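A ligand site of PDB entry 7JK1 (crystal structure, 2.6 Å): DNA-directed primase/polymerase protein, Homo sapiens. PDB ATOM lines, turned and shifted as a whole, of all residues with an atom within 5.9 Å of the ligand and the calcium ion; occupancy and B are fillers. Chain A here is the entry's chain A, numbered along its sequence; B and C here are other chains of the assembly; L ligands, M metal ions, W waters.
A nitrogen (N3) of the ligand sits at hydrogen-bond distance from O6 of 8OG 3 of chain B (3.3 Å).
An oxygen (O11) of the ligand sits at hydrogen-bond distance from the side-chain hydroxyl (OG) of Ser 167, 2.9 Å away.
The backbone NH of Arg 291 sits at hydrogen-bond distance from an oxygen (O3) of the ligand.
An oxygen (O11) of the ligand lies within salt-bridge range of the guanidinium group (NH2) of Arg 291 (2.8 Å).
NZ of Lys 297 is in salt-bridge range of O6 of the ligand.
O13 of the ligand lies within salt-bridge range of NZ of Lys 165, at 2.9 Å.
N3 of the ligand lies close to O6 of DG 12 of chain C (3.3 Å).
A ring nitrogen (NE2) of His 169 lies close to an oxygen (O9) of the ligand (3.4 Å).
NH1 of Arg 288 is in hydrogen-bond range of O2 of the ligand (3.4 Å).
The side-chain carboxylate (OE1) of Glu 116 lies within salt-bridge range of the side-chain amino group (NZ) of Lys 165 (3.8 Å).
The side-chain carboxylate (OD1) of Asp 114 sits close to a ring nitrogen (NE2) of His 169.
O4' of 8OG 3 of chain B sits at hydrogen-bond distance from the backbone NH (N) of Arg 76 (3.1 Å).
The backbone carbonyl oxygen (O) of Ser 167 is in hydrogen-bond range of the backbone NH (N) of Ser 160.
The side-chain hydroxyl of Ser 160 lies within hydrogen-bond range of the guanidinium group of Arg 291.
N3 of DG 12 of chain C is in hydrogen-bond range of NH1 of Arg 288.
N2 of DG 12 of chain C lies close to O2 of DC 4 of chain B (2.7 Å).
The guanidinium group (NH1) of Arg 76 is in hydrogen-bond range of the backbone carbonyl oxygen (O) of Gly 74.
An oxygen (O2) of the ligand sits close to the backbone carbonyl oxygen (O) of Asn 289 (3.4 Å).
NH2 of Arg 76 touches C1 of the ligand (3.6 Å).
CD2 of Tyr 100 touches C6 of the ligand, 3.7 Å away.
Ser 160 touches the ligand.
CG1 of Val 283 touches C9 of the ligand, at 3.9 Å.
Phe 290 touches the ligand.
Of the 23 residues printed, 2 come within 4 Å of the calcium ion.
Along chain A the residues within 4 Å of the calcium ion span positions 114 to 116.
The nearest printed residue that does not touch the calcium ion is Ser 167 (4.004 Å).
The calcium ion is bound by an oxygen (O9) of the ligand (2.0 Å), the side-chain carboxylate (OE2) of Glu 116 (2.3 Å), water W5 (2.3 Å), an oxygen (O5) of the ligand (2.4 Å), the side-chain carboxylate (OD1) of Asp 114 (2.4 Å), the side-chain carboxylate (OD2) of Asp 114 (2.4 Å) and an oxygen (O12) of the ligand (2.6 Å).
Water W5 lies within hydrogen-bond range of the backbone carbonyl oxygen of Leu 115 (2.5 Å), the side-chain hydroxyl of Ser 167 (2.8 Å) and the backbone NH of Arg 168 (3.4 Å).
Water W6 bridges O13 of the ligand and NZ of Lys 165.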
ATOM      1  N   GLY A  74      10.101  -7.812 -23.947  1.00  0.00           N
ATOM      2  CA  GLY A  74      10.796  -8.407 -22.827  1.00  0.00           C
ATOM      3  C   GLY A  74       9.901  -9.160 -21.857  1.00  0.00           C
ATOM      4  O   GLY A  74      10.257  -9.313 -20.679  1.00  0.00           O
ATOM      5  N   ARG A  76       8.522 -11.858 -19.638  1.00  0.00           N
ATOM      6  CA  ARG A  76       9.284 -12.888 -18.971  1.00  0.00           C
ATOM      7  C   ARG A  76       8.380 -13.727 -18.071  1.00  0.00           C
ATOM      8  O   ARG A  76       7.401 -13.229 -17.508  1.00  0.00           O
ATOM      9  CB  ARG A  76      10.404 -12.287 -18.114  1.00  0.00           C
ATOM     10  CG  ARG A  76      11.620 -11.791 -18.904  1.00  0.00           C
ATOM     11  CD  ARG A  76      12.406 -10.766 -18.098  1.00  0.00           C
ATOM     12  NE  ARG A  76      13.770 -10.573 -18.599  1.00  0.00           N
ATOM     13  CZ  ARG A  76      14.080  -9.864 -19.680  1.00  0.00           C
ATOM     14  NH1 ARG A  76      13.126  -9.283 -20.399  1.00  0.00           N
ATOM     15  NH2 ARG A  76      15.345  -9.746 -20.047  1.00  0.00           N
ATOM     16  N   TYR A 100      17.760 -15.489 -17.467  1.00  0.00           N
ATOM     17  CA  TYR A 100      18.319 -14.344 -16.758  1.00  0.00           C
ATOM     18  C   TYR A 100      18.296 -14.612 -15.262  1.00  0.00           C
ATOM     19  O   TYR A 100      17.338 -15.172 -14.735  1.00  0.00           O
ATOM     20  CB  TYR A 100      17.536 -13.059 -17.080  1.00  0.00           C
ATOM     21  CG  TYR A 100      17.554 -12.682 -18.539  1.00  0.00           C
ATOM     22  CD1 TYR A 100      16.667 -13.268 -19.431  1.00  0.00           C
ATOM     23  CD2 TYR A 100      18.454 -11.740 -19.026  1.00  0.00           C
ATOM     24  CE1 TYR A 100      16.684 -12.925 -20.777  1.00  0.00           C
ATOM     25  CE2 TYR A 100      18.467 -11.394 -20.359  1.00  0.00           C
ATOM     26  CZ  TYR A 100      17.579 -11.994 -21.233  1.00  0.00           C
ATOM     27  OH  TYR A 100      17.601 -11.651 -22.562  1.00  0.00           O
ATOM     28  N   ASP A 114      28.446  -4.505 -16.312  1.00  0.00           N
ATOM     29  CA  ASP A 114      27.952  -4.651 -17.676  1.00  0.00           C
ATOM     30  C   ASP A 114      28.681  -3.630 -18.536  1.00  0.00           C
ATOM     31  O   ASP A 114      28.445  -2.425 -18.415  1.00  0.00           O
ATOM     32  CB  ASP A 114      26.437  -4.445 -17.744  1.00  0.00           C
ATOM     33  CG  ASP A 114      25.881  -4.655 -19.139  1.00  0.00           C
ATOM     34  OD1 ASP A 114      25.857  -5.809 -19.599  1.00  0.00           O
ATOM     35  OD2 ASP A 114      25.490  -3.657 -19.777  1.00  0.00           O
ATOM     36  N   LEU A 115      29.583  -4.112 -19.389  1.00  0.00           N
ATOM     37  CA  LEU A 115      30.441  -3.266 -20.200  1.00  0.00           C
ATOM     38  C   LEU A 115      30.042  -3.385 -21.665  1.00  0.00           C
ATOM     39  O   LEU A 115      29.907  -4.499 -22.180  1.00  0.00           O
ATOM     40  CB  LEU A 115      31.910  -3.648 -20.013  1.00  0.00           C
ATOM     41  CG  LEU A 115      32.367  -3.767 -18.562  1.00  0.00           C
ATOM     42  CD1 LEU A 115      33.841  -4.138 -18.490  1.00  0.00           C
ATOM     43  CD2 LEU A 115      32.102  -2.473 -17.789  1.00  0.00           C
ATOM     44  N   GLU A 116      29.853  -2.248 -22.337  1.00  0.00           N
ATOM     45  CA  GLU A 116      29.400  -2.274 -23.711  1.00  0.00           C
ATOM     46  C   GLU A 116      29.668  -0.932 -24.387  1.00  0.00           C
ATOM     47  O   GLU A 116      29.592   0.129 -23.752  1.00  0.00           O
ATOM     48  CB  GLU A 116      27.907  -2.616 -23.797  1.00  0.00           C
ATOM     49  CG  GLU A 116      27.007  -1.682 -22.998  1.00  0.00           C
ATOM     50  CD  GLU A 116      25.541  -2.003 -23.163  1.00  0.00           C
ATOM     51  OE1 GLU A 116      24.724  -1.072 -23.196  1.00  0.00           O
ATOM     52  OE2 GLU A 116      25.209  -3.203 -23.263  1.00  0.00           O
ATOM     53  N   SER A 160      29.984 -11.476 -25.003  1.00  0.00           N
ATOM     54  CA  SER A 160      28.815 -11.730 -25.840  1.00  0.00           C
ATOM     55  C   SER A 160      28.755 -10.706 -26.963  1.00  0.00           C
ATOM     56  O   SER A 160      27.686 -10.244 -27.354  1.00  0.00           O
ATOM     57  CB  SER A 160      27.520 -11.694 -25.012  1.00  0.00           C
ATOM     58  OG  SER A 160      26.390 -11.988 -25.812  1.00  0.00           O
ATOM     59  N   SER A 161      29.923 -10.344 -27.490  1.00  0.00           N
ATOM     60  CA  SER A 161      30.014  -9.293 -28.496  1.00  0.00           C
ATOM     61  C   SER A 161      29.480  -9.775 -29.843  1.00  0.00           C
ATOM     62  O   SER A 161      29.413 -10.975 -30.126  1.00  0.00           O
ATOM     63  CB  SER A 161      31.465  -8.830 -28.655  1.00  0.00           C
ATOM     64  OG  SER A 161      31.991  -8.377 -27.419  1.00  0.00           O
ATOM     65  N   LYS A 165      28.282  -4.662 -31.587  1.00  0.00           N
ATOM     66  CA  LYS A 165      28.328  -4.294 -30.174  1.00  0.00           C
ATOM     67  C   LYS A 165      29.394  -5.117 -29.465  1.00  0.00           C
ATOM     68  O   LYS A 165      29.325  -6.349 -29.437  1.00  0.00           O
ATOM     69  CB  LYS A 165      26.967  -4.520 -29.513  1.00  0.00           C
ATOM     70  CG  LYS A 165      26.909  -4.128 -28.049  1.00  0.00           C
ATOM     71  CD  LYS A 165      25.522  -4.345 -27.483  1.00  0.00           C
ATOM     72  CE  LYS A 165      25.416  -3.857 -26.048  1.00  0.00           C
ATOM     73  NZ  LYS A 165      24.034  -3.959 -25.519  1.00  0.00           N
ATOM     74  N   SER A 167      30.431  -6.416 -26.145  1.00  0.00           N
ATOM     75  CA  SER A 167      29.633  -6.688 -24.949  1.00  0.00           C
ATOM     76  C   SER A 167      30.397  -7.655 -24.050  1.00  0.00           C
ATOM     77  O   SER A 167      30.910  -8.676 -24.517  1.00  0.00           O
ATOM     78  CB  SER A 167      28.276  -7.282 -25.334  1.00  0.00           C
ATOM     79  OG  SER A 167      27.456  -7.469 -24.186  1.00  0.00           O
ATOM     80  N   ARG A 168      30.458  -7.324 -22.754  1.00  0.00           N
ATOM     81  CA  ARG A 168      31.155  -8.173 -21.795  1.00  0.00           C
ATOM     82  C   ARG A 168      30.561  -7.980 -20.402  1.00  0.00           C
ATOM     83  O   ARG A 168      30.161  -6.871 -20.036  1.00  0.00           O
ATOM     84  CB  ARG A 168      32.657  -7.884 -21.771  1.00  0.00           C
ATOM     85  CG  ARG A 168      33.375  -8.288 -23.048  1.00  0.00           C
ATOM     86  CD  ARG A 168      34.876  -8.402 -22.850  1.00  0.00           C
ATOM     87  NE  ARG A 168      35.539  -8.844 -24.077  1.00  0.00           N
ATOM     88  CZ  ARG A 168      36.845  -9.025 -24.193  1.00  0.00           C
ATOM     89  NH1 ARG A 168      37.651  -8.810 -23.154  1.00  0.00           N
ATOM     90  NH2 ARG A 168      37.356  -9.423 -25.345  1.00  0.00           N
ATOM     91  N   HIS A 169      30.517  -9.068 -19.647  1.00  0.00           N
ATOM     92  CA  HIS A 169      30.080  -9.063 -18.252  1.00  0.00           C
ATOM     93  C   HIS A 169      31.238  -9.490 -17.371  1.00  0.00           C
ATOM     94  O   HIS A 169      31.933 -10.461 -17.670  1.00  0.00           O
ATOM     95  CB  HIS A 169      28.887 -10.005 -18.035  1.00  0.00           C
ATOM     96  CG  HIS A 169      27.600  -9.500 -18.603  1.00  0.00           C
ATOM     97  ND1 HIS A 169      26.394 -10.113 -18.358  1.00  0.00           N
ATOM     98  CD2 HIS A 169      27.327  -8.444 -19.402  1.00  0.00           C
ATOM     99  CE1 HIS A 169      25.425  -9.451 -18.984  1.00  0.00           C
ATOM    100  NE2 HIS A 169      25.974  -8.434 -19.626  1.00  0.00           N
ATOM    101  N   ASP A 280      28.068   0.382 -17.814  1.00  0.00           N
ATOM    102  CA  ASP A 280      26.615   0.558 -17.809  1.00  0.00           C
ATOM    103  C   ASP A 280      26.151   0.622 -16.360  1.00  0.00           C
ATOM    104  O   ASP A 280      25.973  -0.407 -15.701  1.00  0.00           O
ATOM    105  CB  ASP A 280      25.940  -0.590 -18.566  1.00  0.00           C
ATOM    106  CG  ASP A 280      24.420  -0.476 -18.580  1.00  0.00           C
ATOM    107  OD1 ASP A 280      23.879   0.444 -17.927  1.00  0.00           O
ATOM    108  OD2 ASP A 280      23.776  -1.311 -19.238  1.00  0.00           O
ATOM    109  N   VAL A 283      22.388  -1.100 -14.479  1.00  0.00           N
ATOM    110  CA  VAL A 283      22.079  -2.479 -14.139  1.00  0.00           C
ATOM    111  C   VAL A 283      22.110  -2.688 -12.621  1.00  0.00           C
ATOM    112  O   VAL A 283      22.265  -3.817 -12.161  1.00  0.00           O
ATOM    113  CB  VAL A 283      23.027  -3.458 -14.843  1.00  0.00           C
ATOM    114  CG1 VAL A 283      22.884  -3.345 -16.350  1.00  0.00           C
ATOM    115  CG2 VAL A 283      24.468  -3.225 -14.409  1.00  0.00           C
ATOM    116  N   ARG A 288      17.089  -6.779 -10.484  1.00  0.00           N
ATOM    117  CA  ARG A 288      17.629  -6.627 -11.821  1.00  0.00           C
ATOM    118  C   ARG A 288      17.834  -7.995 -12.477  1.00  0.00           C
ATOM    119  O   ARG A 288      18.355  -8.926 -11.861  1.00  0.00           O
ATOM    120  CB  ARG A 288      18.962  -5.867 -11.776  1.00  0.00           C
ATOM    121  CG  ARG A 288      19.748  -5.862 -13.082  1.00  0.00           C
ATOM    122  CD  ARG A 288      18.954  -5.267 -14.236  1.00  0.00           C
ATOM    123  NE  ARG A 288      18.632  -3.861 -14.033  1.00  0.00           N
ATOM    124  CZ  ARG A 288      17.961  -3.111 -14.908  1.00  0.00           C
ATOM    125  NH1 ARG A 288      17.546  -3.639 -16.060  1.00  0.00           N
ATOM    126  NH2 ARG A 288      17.710  -1.836 -14.646  1.00  0.00           N
ATOM    127  N   ASN A 289      17.411  -8.095 -13.734  1.00  0.00           N
ATOM    128  CA  ASN A 289      17.662  -9.282 -14.533  1.00  0.00           C
ATOM    129  C   ASN A 289      19.050  -9.182 -15.159  1.00  0.00           C
ATOM    130  O   ASN A 289      19.485  -8.105 -15.562  1.00  0.00           O
ATOM    131  CB  ASN A 289      16.598  -9.443 -15.612  1.00  0.00           C
ATOM    132  CG  ASN A 289      15.282  -9.986 -15.077  1.00  0.00           C
ATOM    133  OD1 ASN A 289      14.665 -10.864 -15.694  1.00  0.00           O
ATOM    134  ND2 ASN A 289      14.852  -9.495 -13.916  1.00  0.00           N
ATOM    135  N   PHE A 290      19.751 -10.308 -15.233  1.00  0.00           N
ATOM    136  CA  PHE A 290      21.111 -10.347 -15.757  1.00  0.00           C
ATOM    137  C   PHE A 290      21.299 -11.652 -16.516  1.00  0.00           C
ATOM    138  O   PHE A 290      21.109 -12.737 -15.949  1.00  0.00           O
ATOM    139  CB  PHE A 290      22.139 -10.200 -14.626  1.00  0.00           C
ATOM    140  CG  PHE A 290      23.382  -9.448 -15.024  1.00  0.00           C
ATOM    141  CD1 PHE A 290      23.300  -8.189 -15.591  1.00  0.00           C
ATOM    142  CD2 PHE A 290      24.640  -9.987 -14.794  1.00  0.00           C
ATOM    143  CE1 PHE A 290      24.435  -7.487 -15.955  1.00  0.00           C
ATOM    144  CE2 PHE A 290      25.785  -9.296 -15.160  1.00  0.00           C
ATOM    145  CZ  PHE A 290      25.680  -8.045 -15.734  1.00  0.00           C
ATOM    146  N   ARG A 291      21.668 -11.542 -17.797  1.00  0.00           N
ATOM    147  CA  ARG A 291      21.670 -12.704 -18.681  1.00  0.00           C
ATOM    148  C   ARG A 291      22.652 -13.756 -18.184  1.00  0.00           C
ATOM    149  O   ARG A 291      23.799 -13.453 -17.830  1.00  0.00           O
ATOM    150  CB  ARG A 291      22.028 -12.265 -20.103  1.00  0.00           C
ATOM    151  CG  ARG A 291      21.821 -13.350 -21.159  1.00  0.00           C
ATOM    152  CD  ARG A 291      21.557 -12.750 -22.534  1.00  0.00           C
ATOM    153  NE  ARG A 291      22.509 -11.693 -22.874  1.00  0.00           N
ATOM    154  CZ  ARG A 291      23.607 -11.849 -23.610  1.00  0.00           C
ATOM    155  NH1 ARG A 291      23.927 -13.047 -24.093  1.00  0.00           N
ATOM    156  NH2 ARG A 291      24.393 -10.810 -23.859  1.00  0.00           N
ATOM    157  N   LYS A 297      20.127 -13.366 -25.815  1.00  0.00           N
ATOM    158  CA  LYS A 297      18.872 -12.621 -25.902  1.00  0.00           C
ATOM    159  C   LYS A 297      17.946 -13.287 -26.922  1.00  0.00           C
ATOM    160  O   LYS A 297      18.401 -13.806 -27.946  1.00  0.00           O
ATOM    161  CB  LYS A 297      19.146 -11.167 -26.293  1.00  0.00           C
ATOM    162  CG  LYS A 297      19.168 -10.219 -25.105  1.00  0.00           C
ATOM    163  CD  LYS A 297      19.737  -8.870 -25.471  1.00  0.00           C
ATOM    164  CE  LYS A 297      19.608  -7.882 -24.322  1.00  0.00           C
ATOM    165  NZ  LYS A 297      20.167  -6.551 -24.680  1.00  0.00           N
ATOM    166  N   LEU A 304      26.408 -15.782 -23.888  1.00  0.00           N
ATOM    167  CA  LEU A 304      27.541 -15.375 -23.071  1.00  0.00           C
ATOM    168  C   LEU A 304      28.463 -16.571 -22.833  1.00  0.00           C
ATOM    169  O   LEU A 304      28.024 -17.626 -22.375  1.00  0.00           O
ATOM    170  CB  LEU A 304      27.052 -14.811 -21.740  1.00  0.00           C
ATOM    171  CG  LEU A 304      26.607 -13.340 -21.791  1.00  0.00           C
ATOM    172  CD1 LEU A 304      25.468 -13.083 -20.823  1.00  0.00           C
ATOM    173  CD2 LEU A 304      27.782 -12.423 -21.491  1.00  0.00           C
ATOM    174  P   8OG B   3       2.789  -9.648 -18.844  1.00  0.00           P
ATOM    175  OP1 8OG B   3       2.175  -8.262 -18.899  1.00  0.00           O
ATOM    176  OP2 8OG B   3       2.997 -10.420 -20.133  1.00  0.00           O
ATOM    177  O5' 8OG B   3       4.201  -9.535 -18.099  1.00  0.00           O
ATOM    178  C5' 8OG B   3       4.843 -10.704 -17.598  1.00  0.00           C
ATOM    179  C4' 8OG B   3       6.030 -10.319 -16.735  1.00  0.00           C
ATOM    180  O4' 8OG B   3       7.160  -9.960 -17.527  1.00  0.00           O
ATOM    181  C3' 8OG B   3       5.724  -9.135 -15.832  1.00  0.00           C
ATOM    182  O3' 8OG B   3       5.711  -9.598 -14.476  1.00  0.00           O
ATOM    183  C2' 8OG B   3       6.850  -8.140 -16.038  1.00  0.00           C
ATOM    184  C1' 8OG B   3       7.854  -8.868 -16.911  1.00  0.00           C
ATOM    185  N9  8OG B   3       8.410  -8.002 -17.984  1.00  0.00           N
ATOM    186  C8  8OG B   3       7.768  -7.479 -19.040  1.00  0.00           C
ATOM    187  N7  8OG B   3       8.505  -6.729 -19.874  1.00  0.00           N
ATOM    188  C5  8OG B   3       9.726  -6.758 -19.342  1.00  0.00           C
ATOM    189  C6  8OG B   3      11.045  -6.177 -19.693  1.00  0.00           C
ATOM    190  O6  8OG B   3      11.180  -5.471 -20.705  1.00  0.00           O
ATOM    191  N1  8OG B   3      12.084  -6.428 -18.882  1.00  0.00           N
ATOM    192  C2  8OG B   3      11.974  -7.187 -17.781  1.00  0.00           C
ATOM    193  N2  8OG B   3      13.081  -7.390 -17.017  1.00  0.00           N
ATOM    194  N3  8OG B   3      10.812  -7.757 -17.393  1.00  0.00           N
ATOM    195  C4  8OG B   3       9.678  -7.587 -18.114  1.00  0.00           C
ATOM    196  O8  8OG B   3       6.517  -7.689 -19.237  1.00  0.00           O
ATOM    197  P    DC B   4       5.380  -8.583 -13.281  1.00  0.00           P
ATOM    198  OP1  DC B   4       5.296  -9.398 -12.037  1.00  0.00           O
ATOM    199  OP2  DC B   4       4.240  -7.739 -13.684  1.00  0.00           O
ATOM    200  O5'  DC B   4       6.687  -7.660 -13.187  1.00  0.00           O
ATOM    201  C5'  DC B   4       7.898  -8.215 -12.719  1.00  0.00           C
ATOM    202  C4'  DC B   4       9.027  -7.199 -12.753  1.00  0.00           C
ATOM    203  O4'  DC B   4       9.272  -6.784 -14.109  1.00  0.00           O
ATOM    204  C3'  DC B   4       8.771  -5.908 -11.976  1.00  0.00           C
ATOM    205  O3'  DC B   4       9.481  -5.928 -10.740  1.00  0.00           O
ATOM    206  C2'  DC B   4       9.274  -4.788 -12.921  1.00  0.00           C
ATOM    207  C1'  DC B   4       9.935  -5.550 -14.052  1.00  0.00           C
ATOM    208  N1   DC B   4       9.845  -4.879 -15.388  1.00  0.00           N
ATOM    209  C2   DC B   4      10.947  -4.177 -15.886  1.00  0.00           C
ATOM    210  O2   DC B   4      11.978  -4.107 -15.204  1.00  0.00           O
ATOM    211  N3   DC B   4      10.860  -3.594 -17.103  1.00  0.00           N
ATOM    212  C4   DC B   4       9.730  -3.693 -17.814  1.00  0.00           C
ATOM    213  N4   DC B   4       9.693  -3.102 -19.008  1.00  0.00           N
ATOM    214  C5   DC B   4       8.607  -4.411 -17.328  1.00  0.00           C
ATOM    215  C6   DC B   4       8.702  -4.984 -16.125  1.00  0.00           C
ATOM    216  P    DG C  12      19.998   1.712 -22.846  1.00  0.00           P
ATOM    217  OP1  DG C  12      21.254   2.471 -22.668  1.00  0.00           O
ATOM    218  OP2  DG C  12      19.731   0.996 -24.113  1.00  0.00           O
ATOM    219  O5'  DG C  12      19.865   0.645 -21.668  1.00  0.00           O
ATOM    220  C5'  DG C  12      20.073   1.050 -20.320  1.00  0.00           C
ATOM    221  C4'  DG C  12      19.960  -0.134 -19.386  1.00  0.00           C
ATOM    222  O4'  DG C  12      18.557  -0.434 -19.144  1.00  0.00           O
ATOM    223  C3'  DG C  12      20.584  -1.431 -19.917  1.00  0.00           C
ATOM    224  O3'  DG C  12      21.308  -2.104 -18.894  1.00  0.00           O
ATOM    225  C2'  DG C  12      19.384  -2.223 -20.420  1.00  0.00           C
ATOM    226  C1'  DG C  12      18.290  -1.786 -19.458  1.00  0.00           C
ATOM    227  N9   DG C  12      16.935  -1.885 -20.003  1.00  0.00           N
ATOM    228  C8   DG C  12      16.535  -1.614 -21.289  1.00  0.00           C
ATOM    229  N7   DG C  12      15.258  -1.791 -21.478  1.00  0.00           N
ATOM    230  C5   DG C  12      14.781  -2.214 -20.247  1.00  0.00           C
ATOM    231  C6   DG C  12      13.471  -2.554 -19.850  1.00  0.00           C
ATOM    232  O6   DG C  12      12.435  -2.563 -20.531  1.00  0.00           O
ATOM    233  N1   DG C  12      13.423  -2.931 -18.508  1.00  0.00           N
ATOM    234  C2   DG C  12      14.502  -2.968 -17.666  1.00  0.00           C
ATOM    235  N2   DG C  12      14.258  -3.353 -16.399  1.00  0.00           N
ATOM    236  N3   DG C  12      15.735  -2.644 -18.025  1.00  0.00           N
ATOM    237  C4   DG C  12      15.797  -2.282 -19.328  1.00  0.00           C
HETATM  238  N1  LIG L   1      17.082  -6.269 -19.126  1.00  0.00           N
HETATM  239  C1  LIG L   1      15.710  -6.334 -18.815  1.00  0.00           C
HETATM  240  N2  LIG L   1      14.798  -5.902 -19.718  1.00  0.00           N
HETATM  241  C2  LIG L   1      15.189  -5.418 -20.915  1.00  0.00           C
HETATM  242  C3  LIG L   1      16.538  -5.353 -21.227  1.00  0.00           C
HETATM  243  C4  LIG L   1      17.477  -5.793 -20.313  1.00  0.00           C
HETATM  244  O1  LIG L   1      15.346  -6.783 -17.714  1.00  0.00           O
HETATM  245  N3  LIG L   1      14.276  -4.986 -21.819  1.00  0.00           N
HETATM  246  C5  LIG L   1      18.097  -6.739 -18.172  1.00  0.00           C
HETATM  247  C6  LIG L   1      18.649  -8.068 -18.662  1.00  0.00           C
HETATM  248  C7  LIG L   1      20.080  -7.770 -19.084  1.00  0.00           C
HETATM  249  C8  LIG L   1      20.429  -6.478 -18.356  1.00  0.00           C
HETATM  250  O2  LIG L   1      19.189  -5.813 -18.101  1.00  0.00           O
HETATM  251  O3  LIG L   1      20.938  -8.852 -18.716  1.00  0.00           O
HETATM  252  C9  LIG L   1      21.345  -5.578 -19.187  1.00  0.00           C
HETATM  253  O4  LIG L   1      20.762  -5.387 -20.468  1.00  0.00           O
HETATM  254  P1  LIG L   1      21.677  -5.224 -21.783  1.00  0.00           P
HETATM  255  O5  LIG L   1      23.074  -4.823 -21.391  1.00  0.00           O
HETATM  256  O6  LIG L   1      20.901  -4.405 -22.786  1.00  0.00           O
HETATM  257  O7  LIG L   1      21.711  -6.747 -22.300  1.00  0.00           O
HETATM  258  P2  LIG L   1      23.073  -7.583 -22.156  1.00  0.00           P
HETATM  259  O8  LIG L   1      22.807  -8.714 -21.195  1.00  0.00           O
HETATM  260  O9  LIG L   1      24.199  -6.623 -21.897  1.00  0.00           O
HETATM  261  O10 LIG L   1      23.241  -8.187 -23.637  1.00  0.00           O
HETATM  262  P3  LIG L   1      24.147  -7.402 -24.717  1.00  0.00           P
HETATM  263  O11 LIG L   1      24.969  -8.477 -25.377  1.00  0.00           O
HETATM  264  O12 LIG L   1      24.946  -6.417 -23.890  1.00  0.00           O
HETATM  265  O13 LIG L   1      23.114  -6.756 -25.606  1.00  0.00           O
HETATM  266 CA    CA M   1      25.390  -5.003 -21.803  1.00  0.00          CA
HETATM  267  O   HOH W   1      15.355  -6.028 -14.996  1.00  0.00           O
HETATM  268  O   HOH W   2      16.565  -8.296 -21.732  1.00  0.00           O
HETATM  269  O   HOH W   3      16.435  -6.896 -23.993  1.00  0.00           O
HETATM  270  O   HOH W   4      24.154  -9.699 -27.374  1.00  0.00           O
HETATM  271  O   HOH W   5      27.642  -5.556 -22.116  1.00  0.00           O
HETATM  272  O   HOH W   6      22.984  -5.757 -27.999  1.00  0.00           O
